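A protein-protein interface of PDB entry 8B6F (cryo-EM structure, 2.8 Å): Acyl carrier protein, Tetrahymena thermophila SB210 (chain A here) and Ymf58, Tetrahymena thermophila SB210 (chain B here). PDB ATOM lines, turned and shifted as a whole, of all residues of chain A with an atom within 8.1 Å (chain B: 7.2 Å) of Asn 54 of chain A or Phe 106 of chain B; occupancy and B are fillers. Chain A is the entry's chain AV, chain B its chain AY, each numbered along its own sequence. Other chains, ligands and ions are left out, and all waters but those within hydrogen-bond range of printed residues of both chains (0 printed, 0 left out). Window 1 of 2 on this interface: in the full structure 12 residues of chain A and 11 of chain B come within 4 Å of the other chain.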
ATOM      1  N   SER A  40      14.303   3.490 -28.001  1.00  0.00           N
ATOM      2  CA  SER A  40      15.119   4.370 -28.832  1.00  0.00           C
ATOM      3  C   SER A  40      14.451   5.719 -29.074  1.00  0.00           C
ATOM      4  O   SER A  40      14.816   6.425 -30.017  1.00  0.00           O
ATOM      5  CB  SER A  40      15.438   3.694 -30.167  1.00  0.00           C
ATOM      6  OG  SER A  40      14.254   3.410 -30.890  1.00  0.00           O
ATOM      7  N   THR A  42      13.774   9.550 -28.621  1.00  0.00           N
ATOM      8  CA  THR A  42      14.530  10.720 -28.202  1.00  0.00           C
ATOM      9  C   THR A  42      13.762  11.982 -28.560  1.00  0.00           C
ATOM     10  O   THR A  42      13.025  12.024 -29.547  1.00  0.00           O
ATOM     11  CB  THR A  42      15.918  10.761 -28.851  1.00  0.00           C
ATOM     12  OG1 THR A  42      15.780  10.794 -30.277  1.00  0.00           O
ATOM     13  CG2 THR A  42      16.731   9.542 -28.454  1.00  0.00           C
ATOM     14  N   HIS A  45      14.909  13.945 -32.190  1.00  0.00           N
ATOM     15  CA  HIS A  45      14.536  13.390 -33.488  1.00  0.00           C
ATOM     16  C   HIS A  45      13.021  13.232 -33.557  1.00  0.00           C
ATOM     17  O   HIS A  45      12.449  12.370 -32.884  1.00  0.00           O
ATOM     18  CB  HIS A  45      15.233  12.052 -33.716  1.00  0.00           C
ATOM     19  CG  HIS A  45      16.725  12.135 -33.666  1.00  0.00           C
ATOM     20  ND1 HIS A  45      17.428  12.206 -32.483  1.00  0.00           N
ATOM     21  CD2 HIS A  45      17.648  12.167 -34.654  1.00  0.00           C
ATOM     22  CE1 HIS A  45      18.721  12.275 -32.745  1.00  0.00           C
ATOM     23  NE2 HIS A  45      18.882  12.253 -34.055  1.00  0.00           N
ATOM     24  N   LYS A  49      14.685   7.089 -34.554  1.00  0.00           N
ATOM     25  CA  LYS A  49      15.849   6.380 -35.057  1.00  0.00           C
ATOM     26  C   LYS A  49      15.572   4.882 -35.132  1.00  0.00           C
ATOM     27  O   LYS A  49      14.705   4.344 -34.439  1.00  0.00           O
ATOM     28  CB  LYS A  49      17.061   6.648 -34.167  1.00  0.00           C
ATOM     29  CG  LYS A  49      17.531   8.094 -34.194  1.00  0.00           C
ATOM     30  CD  LYS A  49      18.030   8.550 -32.832  1.00  0.00           C
ATOM     31  CE  LYS A  49      19.201   7.713 -32.345  1.00  0.00           C
ATOM     32  NZ  LYS A  49      19.710   8.198 -31.030  1.00  0.00           N
ATOM     33  N   ASN A  51      17.453   2.318 -34.205  1.00  0.00           N
ATOM     34  CA  ASN A  51      17.849   1.548 -33.036  1.00  0.00           C
ATOM     35  C   ASN A  51      18.520   2.463 -32.025  1.00  0.00           C
ATOM     36  O   ASN A  51      18.929   3.584 -32.341  1.00  0.00           O
ATOM     37  CB  ASN A  51      18.783   0.393 -33.414  1.00  0.00           C
ATOM     38  CG  ASN A  51      20.001   0.856 -34.186  1.00  0.00           C
ATOM     39  OD1 ASN A  51      20.341   2.037 -34.183  1.00  0.00           O
ATOM     40  ND2 ASN A  51      20.666  -0.078 -34.854  1.00  0.00           N
ATOM     41  N   LYS A  52      18.624   1.964 -30.791  1.00  0.00           N
ATOM     42  CA  LYS A  52      19.262   2.716 -29.718  1.00  0.00           C
ATOM     43  C   LYS A  52      20.744   2.947 -29.977  1.00  0.00           C
ATOM     44  O   LYS A  52      21.330   3.860 -29.386  1.00  0.00           O
ATOM     45  CB  LYS A  52      19.069   1.977 -28.394  1.00  0.00           C
ATOM     46  CG  LYS A  52      19.657   2.672 -27.179  1.00  0.00           C
ATOM     47  CD  LYS A  52      19.410   1.852 -25.925  1.00  0.00           C
ATOM     48  CE  LYS A  52      19.990   2.524 -24.695  1.00  0.00           C
ATOM     49  NZ  LYS A  52      19.789   1.699 -23.471  1.00  0.00           N
ATOM     50  N   PHE A  53      21.361   2.146 -30.842  1.00  0.00           N
ATOM     51  CA  PHE A  53      22.788   2.277 -31.111  1.00  0.00           C
ATOM     52  C   PHE A  53      23.034   3.520 -31.955  1.00  0.00           C
ATOM     53  O   PHE A  53      22.527   3.629 -33.076  1.00  0.00           O
ATOM     54  CB  PHE A  53      23.310   1.034 -31.830  1.00  0.00           C
ATOM     55  CG  PHE A  53      22.810  -0.256 -31.251  1.00  0.00           C
ATOM     56  CD1 PHE A  53      22.614  -0.394 -29.886  1.00  0.00           C
ATOM     57  CD2 PHE A  53      22.526  -1.330 -32.076  1.00  0.00           C
ATOM     58  CE1 PHE A  53      22.150  -1.579 -29.355  1.00  0.00           C
ATOM     59  CE2 PHE A  53      22.061  -2.518 -31.552  1.00  0.00           C
ATOM     60  CZ  PHE A  53      21.872  -2.644 -30.190  1.00  0.00           C
ATOM     61  N   ASN A  54      23.818   4.453 -31.424  1.00  0.00           N
ATOM     62  CA  ASN A  54      24.120   5.699 -32.127  1.00  0.00           C
ATOM     63  C   ASN A  54      25.330   5.516 -33.045  1.00  0.00           C
ATOM     64  O   ASN A  54      26.350   6.191 -32.929  1.00  0.00           O
ATOM     65  CB  ASN A  54      24.352   6.823 -31.125  1.00  0.00           C
ATOM     66  CG  ASN A  54      23.100   7.188 -30.363  1.00  0.00           C
ATOM     67  OD1 ASN A  54      21.992   7.094 -30.888  1.00  0.00           O
ATOM     68  ND2 ASN A  54      23.268   7.604 -29.115  1.00  0.00           N
ATOM     69  N   THR A  55      25.195   4.576 -33.980  1.00  0.00           N
ATOM     70  CA  THR A  55      26.245   4.274 -34.945  1.00  0.00           C
ATOM     71  C   THR A  55      25.910   4.790 -36.340  1.00  0.00           C
ATOM     72  O   THR A  55      26.505   4.338 -37.324  1.00  0.00           O
ATOM     73  CB  THR A  55      26.507   2.768 -34.991  1.00  0.00           C
ATOM     74  OG1 THR A  55      25.294   2.074 -35.315  1.00  0.00           O
ATOM     75  CG2 THR A  55      27.030   2.277 -33.651  1.00  0.00           C
ATOM     76  N   GLU A  56      24.971   5.725 -36.446  1.00  0.00           N
ATOM     77  CA  GLU A  56      24.606   6.270 -37.746  1.00  0.00           C
ATOM     78  C   GLU A  56      25.795   6.989 -38.369  1.00  0.00           C
ATOM     79  O   GLU A  56      26.577   7.648 -37.677  1.00  0.00           O
ATOM     80  CB  GLU A  56      23.428   7.231 -37.604  1.00  0.00           C
ATOM     81  CG  GLU A  56      22.186   6.603 -36.993  1.00  0.00           C
ATOM     82  CD  GLU A  56      21.045   7.594 -36.849  1.00  0.00           C
ATOM     83  OE1 GLU A  56      21.286   8.808 -37.023  1.00  0.00           O
ATOM     84  OE2 GLU A  56      19.907   7.160 -36.568  1.00  0.00           O
ATOM     85  N   THR A  57      25.926   6.861 -39.685  1.00  0.00           N
ATOM     86  CA  THR A  57      27.002   7.485 -40.437  1.00  0.00           C
ATOM     87  C   THR A  57      26.419   8.412 -41.494  1.00  0.00           C
ATOM     88  O   THR A  57      25.272   8.258 -41.922  1.00  0.00           O
ATOM     89  CB  THR A  57      27.903   6.439 -41.110  1.00  0.00           C
ATOM     90  OG1 THR A  57      27.118   5.611 -41.978  1.00  0.00           O
ATOM     91  CG2 THR A  57      28.590   5.571 -40.067  1.00  0.00           C
ATOM     92  N   ILE A 135      32.077   7.041 -37.646  1.00  0.00           N
ATOM     93  CA  ILE A 135      30.754   7.177 -37.048  1.00  0.00           C
ATOM     94  C   ILE A 135      30.601   8.460 -36.238  1.00  0.00           C
ATOM     95  O   ILE A 135      29.463   8.872 -35.967  1.00  0.00           O
ATOM     96  CB  ILE A 135      30.416   5.959 -36.160  1.00  0.00           C
ATOM     97  CG1 ILE A 135      31.367   5.888 -34.961  1.00  0.00           C
ATOM     98  CG2 ILE A 135      30.477   4.680 -36.984  1.00  0.00           C
ATOM     99  CD1 ILE A 135      31.058   4.769 -33.988  1.00  0.00           C
ATOM    100  N   ASN A 136      31.701   9.094 -35.834  1.00  0.00           N
ATOM    101  CA  ASN A 136      31.627  10.296 -35.015  1.00  0.00           C
ATOM    102  C   ASN A 136      31.409  11.563 -35.829  1.00  0.00           C
ATOM    103  O   ASN A 136      31.159  12.618 -35.238  1.00  0.00           O
ATOM    104  CB  ASN A 136      32.907  10.447 -34.192  1.00  0.00           C
ATOM    105  CG  ASN A 136      33.208   9.226 -33.353  1.00  0.00           C
ATOM    106  OD1 ASN A 136      32.607   9.016 -32.303  1.00  0.00           O
ATOM    107  ND2 ASN A 136      34.152   8.414 -33.812  1.00  0.00           N
ATOM    108  N   ASP B  91      20.834  11.009 -14.106  1.00  0.00           N
ATOM    109  CA  ASP B  91      20.237  10.500 -15.334  1.00  0.00           C
ATOM    110  C   ASP B  91      21.260  10.317 -16.446  1.00  0.00           C
ATOM    111  O   ASP B  91      20.996   9.575 -17.397  1.00  0.00           O
ATOM    112  CB  ASP B  91      19.123  11.440 -15.800  1.00  0.00           C
ATOM    113  CG  ASP B  91      19.589  12.876 -15.922  1.00  0.00           C
ATOM    114  OD1 ASP B  91      20.363  13.174 -16.855  1.00  0.00           O
ATOM    115  OD2 ASP B  91      19.182  13.706 -15.082  1.00  0.00           O
ATOM    116  N   LEU B  92      22.416  10.969 -16.355  1.00  0.00           N
ATOM    117  CA  LEU B  92      23.471  10.824 -17.348  1.00  0.00           C
ATOM    118  C   LEU B  92      24.432   9.687 -17.034  1.00  0.00           C
ATOM    119  O   LEU B  92      25.383   9.474 -17.792  1.00  0.00           O
ATOM    120  CB  LEU B  92      24.261  12.132 -17.477  1.00  0.00           C
ATOM    121  CG  LEU B  92      23.515  13.346 -18.039  1.00  0.00           C
ATOM    122  CD1 LEU B  92      24.425  14.560 -18.036  1.00  0.00           C
ATOM    123  CD2 LEU B  92      22.994  13.078 -19.442  1.00  0.00           C
ATOM    124  N   ASN B  93      24.215   8.959 -15.943  1.00  0.00           N
ATOM    125  CA  ASN B  93      25.076   7.847 -15.565  1.00  0.00           C
ATOM    126  C   ASN B  93      24.628   6.524 -16.167  1.00  0.00           C
ATOM    127  O   ASN B  93      25.235   5.490 -15.872  1.00  0.00           O
ATOM    128  CB  ASN B  93      25.131   7.719 -14.039  1.00  0.00           C
ATOM    129  CG  ASN B  93      25.757   8.928 -13.376  1.00  0.00           C
ATOM    130  OD1 ASN B  93      26.580   9.619 -13.972  1.00  0.00           O
ATOM    131  ND2 ASN B  93      25.370   9.188 -12.133  1.00  0.00           N
ATOM    132  N   ASN B  94      23.585   6.529 -16.992  1.00  0.00           N
ATOM    133  CA  ASN B  94      23.105   5.329 -17.656  1.00  0.00           C
ATOM    134  C   ASN B  94      22.753   5.670 -19.095  1.00  0.00           C
ATOM    135  O   ASN B  94      22.508   6.829 -19.438  1.00  0.00           O
ATOM    136  CB  ASN B  94      21.892   4.729 -16.934  1.00  0.00           C
ATOM    137  CG  ASN B  94      20.811   5.752 -16.666  1.00  0.00           C
ATOM    138  OD1 ASN B  94      20.053   6.118 -17.561  1.00  0.00           O
ATOM    139  ND2 ASN B  94      20.732   6.216 -15.426  1.00  0.00           N
ATOM    140  N   ASN B  95      22.740   4.643 -19.939  1.00  0.00           N
ATOM    141  CA  ASN B  95      22.500   4.804 -21.365  1.00  0.00           C
ATOM    142  C   ASN B  95      21.024   4.739 -21.734  1.00  0.00           C
ATOM    143  O   ASN B  95      20.689   4.912 -22.909  1.00  0.00           O
ATOM    144  CB  ASN B  95      23.271   3.736 -22.146  1.00  0.00           C
ATOM    145  CG  ASN B  95      23.323   4.023 -23.629  1.00  0.00           C
ATOM    146  OD1 ASN B  95      23.125   5.157 -24.060  1.00  0.00           O
ATOM    147  ND2 ASN B  95      23.593   2.993 -24.423  1.00  0.00           N
ATOM    148  N   ASN B  96      20.139   4.498 -20.770  1.00  0.00           N
ATOM    149  CA  ASN B  96      18.715   4.430 -21.066  1.00  0.00           C
ATOM    150  C   ASN B  96      18.244   5.730 -21.702  1.00  0.00           C
ATOM    151  O   ASN B  96      18.530   6.820 -21.200  1.00  0.00           O
ATOM    152  CB  ASN B  96      17.923   4.158 -19.787  1.00  0.00           C
ATOM    153  CG  ASN B  96      18.348   2.878 -19.097  1.00  0.00           C
ATOM    154  OD1 ASN B  96      18.921   1.985 -19.717  1.00  0.00           O
ATOM    155  ND2 ASN B  96      18.059   2.782 -17.806  1.00  0.00           N
ATOM    156  N   ASN B  97      17.519   5.613 -22.811  1.00  0.00           N
ATOM    157  CA  ASN B  97      17.005   6.795 -23.487  1.00  0.00           C
ATOM    158  C   ASN B  97      15.952   7.479 -22.628  1.00  0.00           C
ATOM    159  O   ASN B  97      15.124   6.823 -21.990  1.00  0.00           O
ATOM    160  CB  ASN B  97      16.415   6.425 -24.848  1.00  0.00           C
ATOM    161  CG  ASN B  97      17.480   6.214 -25.905  1.00  0.00           C
ATOM    162  OD1 ASN B  97      18.603   5.817 -25.602  1.00  0.00           O
ATOM    163  ND2 ASN B  97      17.134   6.494 -27.155  1.00  0.00           N
ATOM    164  N   ASP B 103      19.493  16.494 -24.920  1.00  0.00           N
ATOM    165  CA  ASP B 103      20.768  16.191 -25.566  1.00  0.00           C
ATOM    166  C   ASP B 103      21.463  15.014 -24.895  1.00  0.00           C
ATOM    167  O   ASP B 103      22.659  15.056 -24.601  1.00  0.00           O
ATOM    168  CB  ASP B 103      21.678  17.415 -25.553  1.00  0.00           C
ATOM    169  CG  ASP B 103      22.041  17.853 -24.149  1.00  0.00           C
ATOM    170  OD1 ASP B 103      21.250  17.591 -23.220  1.00  0.00           O
ATOM    171  OD2 ASP B 103      23.117  18.461 -23.975  1.00  0.00           O
ATOM    172  N   LYS B 104      20.725  13.938 -24.642  1.00  0.00           N
ATOM    173  CA  LYS B 104      21.318  12.708 -24.133  1.00  0.00           C
ATOM    174  C   LYS B 104      21.673  11.815 -25.316  1.00  0.00           C
ATOM    175  O   LYS B 104      20.790  11.391 -26.068  1.00  0.00           O
ATOM    176  CB  LYS B 104      20.365  11.991 -23.178  1.00  0.00           C
ATOM    177  CG  LYS B 104      20.991  10.793 -22.476  1.00  0.00           C
ATOM    178  CD  LYS B 104      20.068  10.228 -21.409  1.00  0.00           C
ATOM    179  CE  LYS B 104      20.706   9.047 -20.694  1.00  0.00           C
ATOM    180  NZ  LYS B 104      19.824   8.502 -19.625  1.00  0.00           N
ATOM    181  N   ASN B 105      22.964  11.539 -25.481  1.00  0.00           N
ATOM    182  CA  ASN B 105      23.442  10.765 -26.624  1.00  0.00           C
ATOM    183  C   ASN B 105      24.805  10.194 -26.274  1.00  0.00           C
ATOM    184  O   ASN B 105      25.748  10.955 -26.038  1.00  0.00           O
ATOM    185  CB  ASN B 105      23.522  11.647 -27.874  1.00  0.00           C
ATOM    186  CG  ASN B 105      23.936  10.877 -29.114  1.00  0.00           C
ATOM    187  OD1 ASN B 105      24.732   9.941 -29.046  1.00  0.00           O
ATOM    188  ND2 ASN B 105      23.400  11.276 -30.261  1.00  0.00           N
ATOM    189  N   PHE B 106      24.911   8.866 -26.245  1.00  0.00           N
ATOM    190  CA  PHE B 106      26.159   8.179 -25.945  1.00  0.00           C
ATOM    191  C   PHE B 106      26.487   7.196 -27.057  1.00  0.00           C
ATOM    192  O   PHE B 106      25.598   6.528 -27.592  1.00  0.00           O
ATOM    193  CB  PHE B 106      26.083   7.434 -24.605  1.00  0.00           C
ATOM    194  CG  PHE B 106      25.994   8.335 -23.407  1.00  0.00           C
ATOM    195  CD1 PHE B 106      26.714   9.517 -23.349  1.00  0.00           C
ATOM    196  CD2 PHE B 106      25.192   7.994 -22.333  1.00  0.00           C
ATOM    197  CE1 PHE B 106      26.631  10.341 -22.245  1.00  0.00           C
ATOM    198  CE2 PHE B 106      25.106   8.813 -21.227  1.00  0.00           C
ATOM    199  CZ  PHE B 106      25.826   9.988 -21.183  1.00  0.00           C
ATOM    200  N   LYS B 107      27.770   7.114 -27.396  1.00  0.00           N
ATOM    201  CA  LYS B 107      28.275   6.181 -28.389  1.00  0.00           C
ATOM    202  C   LYS B 107      29.387   5.353 -27.768  1.00  0.00           C
ATOM    203  O   LYS B 107      30.024   5.762 -26.796  1.00  0.00           O
ATOM    204  CB  LYS B 107      28.813   6.902 -29.634  1.00  0.00           C
ATOM    205  CG  LYS B 107      27.774   7.674 -30.422  1.00  0.00           C
ATOM    206  CD  LYS B 107      28.423   8.483 -31.534  1.00  0.00           C
ATOM    207  CE  LYS B 107      27.385   9.140 -32.431  1.00  0.00           C
ATOM    208  NZ  LYS B 107      26.372   9.914 -31.663  1.00  0.00           N
ATOM    209  N   THR B 108      29.615   4.179 -28.339  1.00  0.00           N
ATOM    210  CA  THR B 108      30.756   3.382 -27.922  1.00  0.00           C
ATOM    211  C   THR B 108      32.042   4.133 -28.260  1.00  0.00           C
ATOM    212  O   THR B 108      32.114   4.801 -29.298  1.00  0.00           O
ATOM    213  CB  THR B 108      30.750   2.020 -28.614  1.00  0.00           C
ATOM    214  OG1 THR B 108      31.890   1.261 -28.195  1.00  0.00           O
ATOM    215  CG2 THR B 108      30.793   2.188 -30.124  1.00  0.00           C
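The backbone carbonyl oxygen of Asn 95 of chain B sits close to the side-chain amino group of Lys 52 of chain A (3.4 Å). ND2 of Asn 54 of chain A sits at hydrogen-bond distance from OD1 of Asn 105 of chain B (2.8 Å). O of Phe 106 of chain B is in hydrogen-bond range of ND2 of Asn 54 of chain A.
ND1 of His 45 of chain A lies within hydrogen-bond range of OG1 of Thr 42 of chain A, 3.1 Å away. The side-chain amide oxygen of Asn 54 of chain A is in hydrogen-bond range of the side-chain amino group of Lys 49 of chain A (2.5 Å). O of Asn 96 of chain B is in hydrogen-bond range of NZ of Lys 104 of chain B (2.6 Å). The side-chain amino group of Lys 107 of chain B is in hydrogen-bond range of the side-chain amide oxygen of Asn 105 of chain B (3.1 Å).
Ser 40 of chain A touches Asn 97 of chain B. Thr 42 of chain A touches Asn 97 of chain B (CG2 to ND2, 3.3 Å). Lys 52 of chain A touches Asn 96 of chain B (NZ to CA, 3.8 Å). OD1 of Asn 97 of chain B touches CG of Lys 52 of chain A (3.7 Å). CE of Lys 107 of chain B touches O of Asn 54 of chain A, at 3.2 Å.
Asn 54 of chain A touches three residues of chain B. Phe 106 of chain B touches just one residue of chain A: Asn 54. Of the printed residues of chain A, Asn 105 of chain B touches Asn 54 (2.8 Å). Of the printed residues of chain B, Thr 42 of chain A touches Asn 97 (3.3 Å). Printed residues of chain A within 4 Å of Asn 95 of chain B: Lys 52 (3.1 Å). Of the printed residues of chain A, Asn 96 of chain B touches Lys 52 (3.8 Å). Of the printed residues of chain B, Ser 40 of chain A touches Asn 97 (3.4 Å). Printed residues of chain A within 4 Å of Asn 97 of chain B: Ser 40, Thr 42 and Lys 52. Asn 94 of chain B touches none of the printed residues of chain A. The nearest residue of chain B that does not touch Asn 54 of chain A is Lys 104 of chain B (5.5 Å). The nearest printed residue of chain B that does not touch Thr 42 of chain A is Lys 104 of chain B (5.1 Å).
Printed residues of chain A that touch a printed residue of chain B: Ser 40, Thr 42, Lys 52 and Asn 54. Of the 13 printed residues of chain B, 6 touch a printed residue of chain A. Along chain B the printed residues that touch a printed residue of chain A span positions 95 to 107. Among the printed residues, 8 pairs touch across the chains. Among the printed residues, no Asp or Glu carboxylate lies within 4 Å of a Lys or Arg side-chain nitrogen of the other chain.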
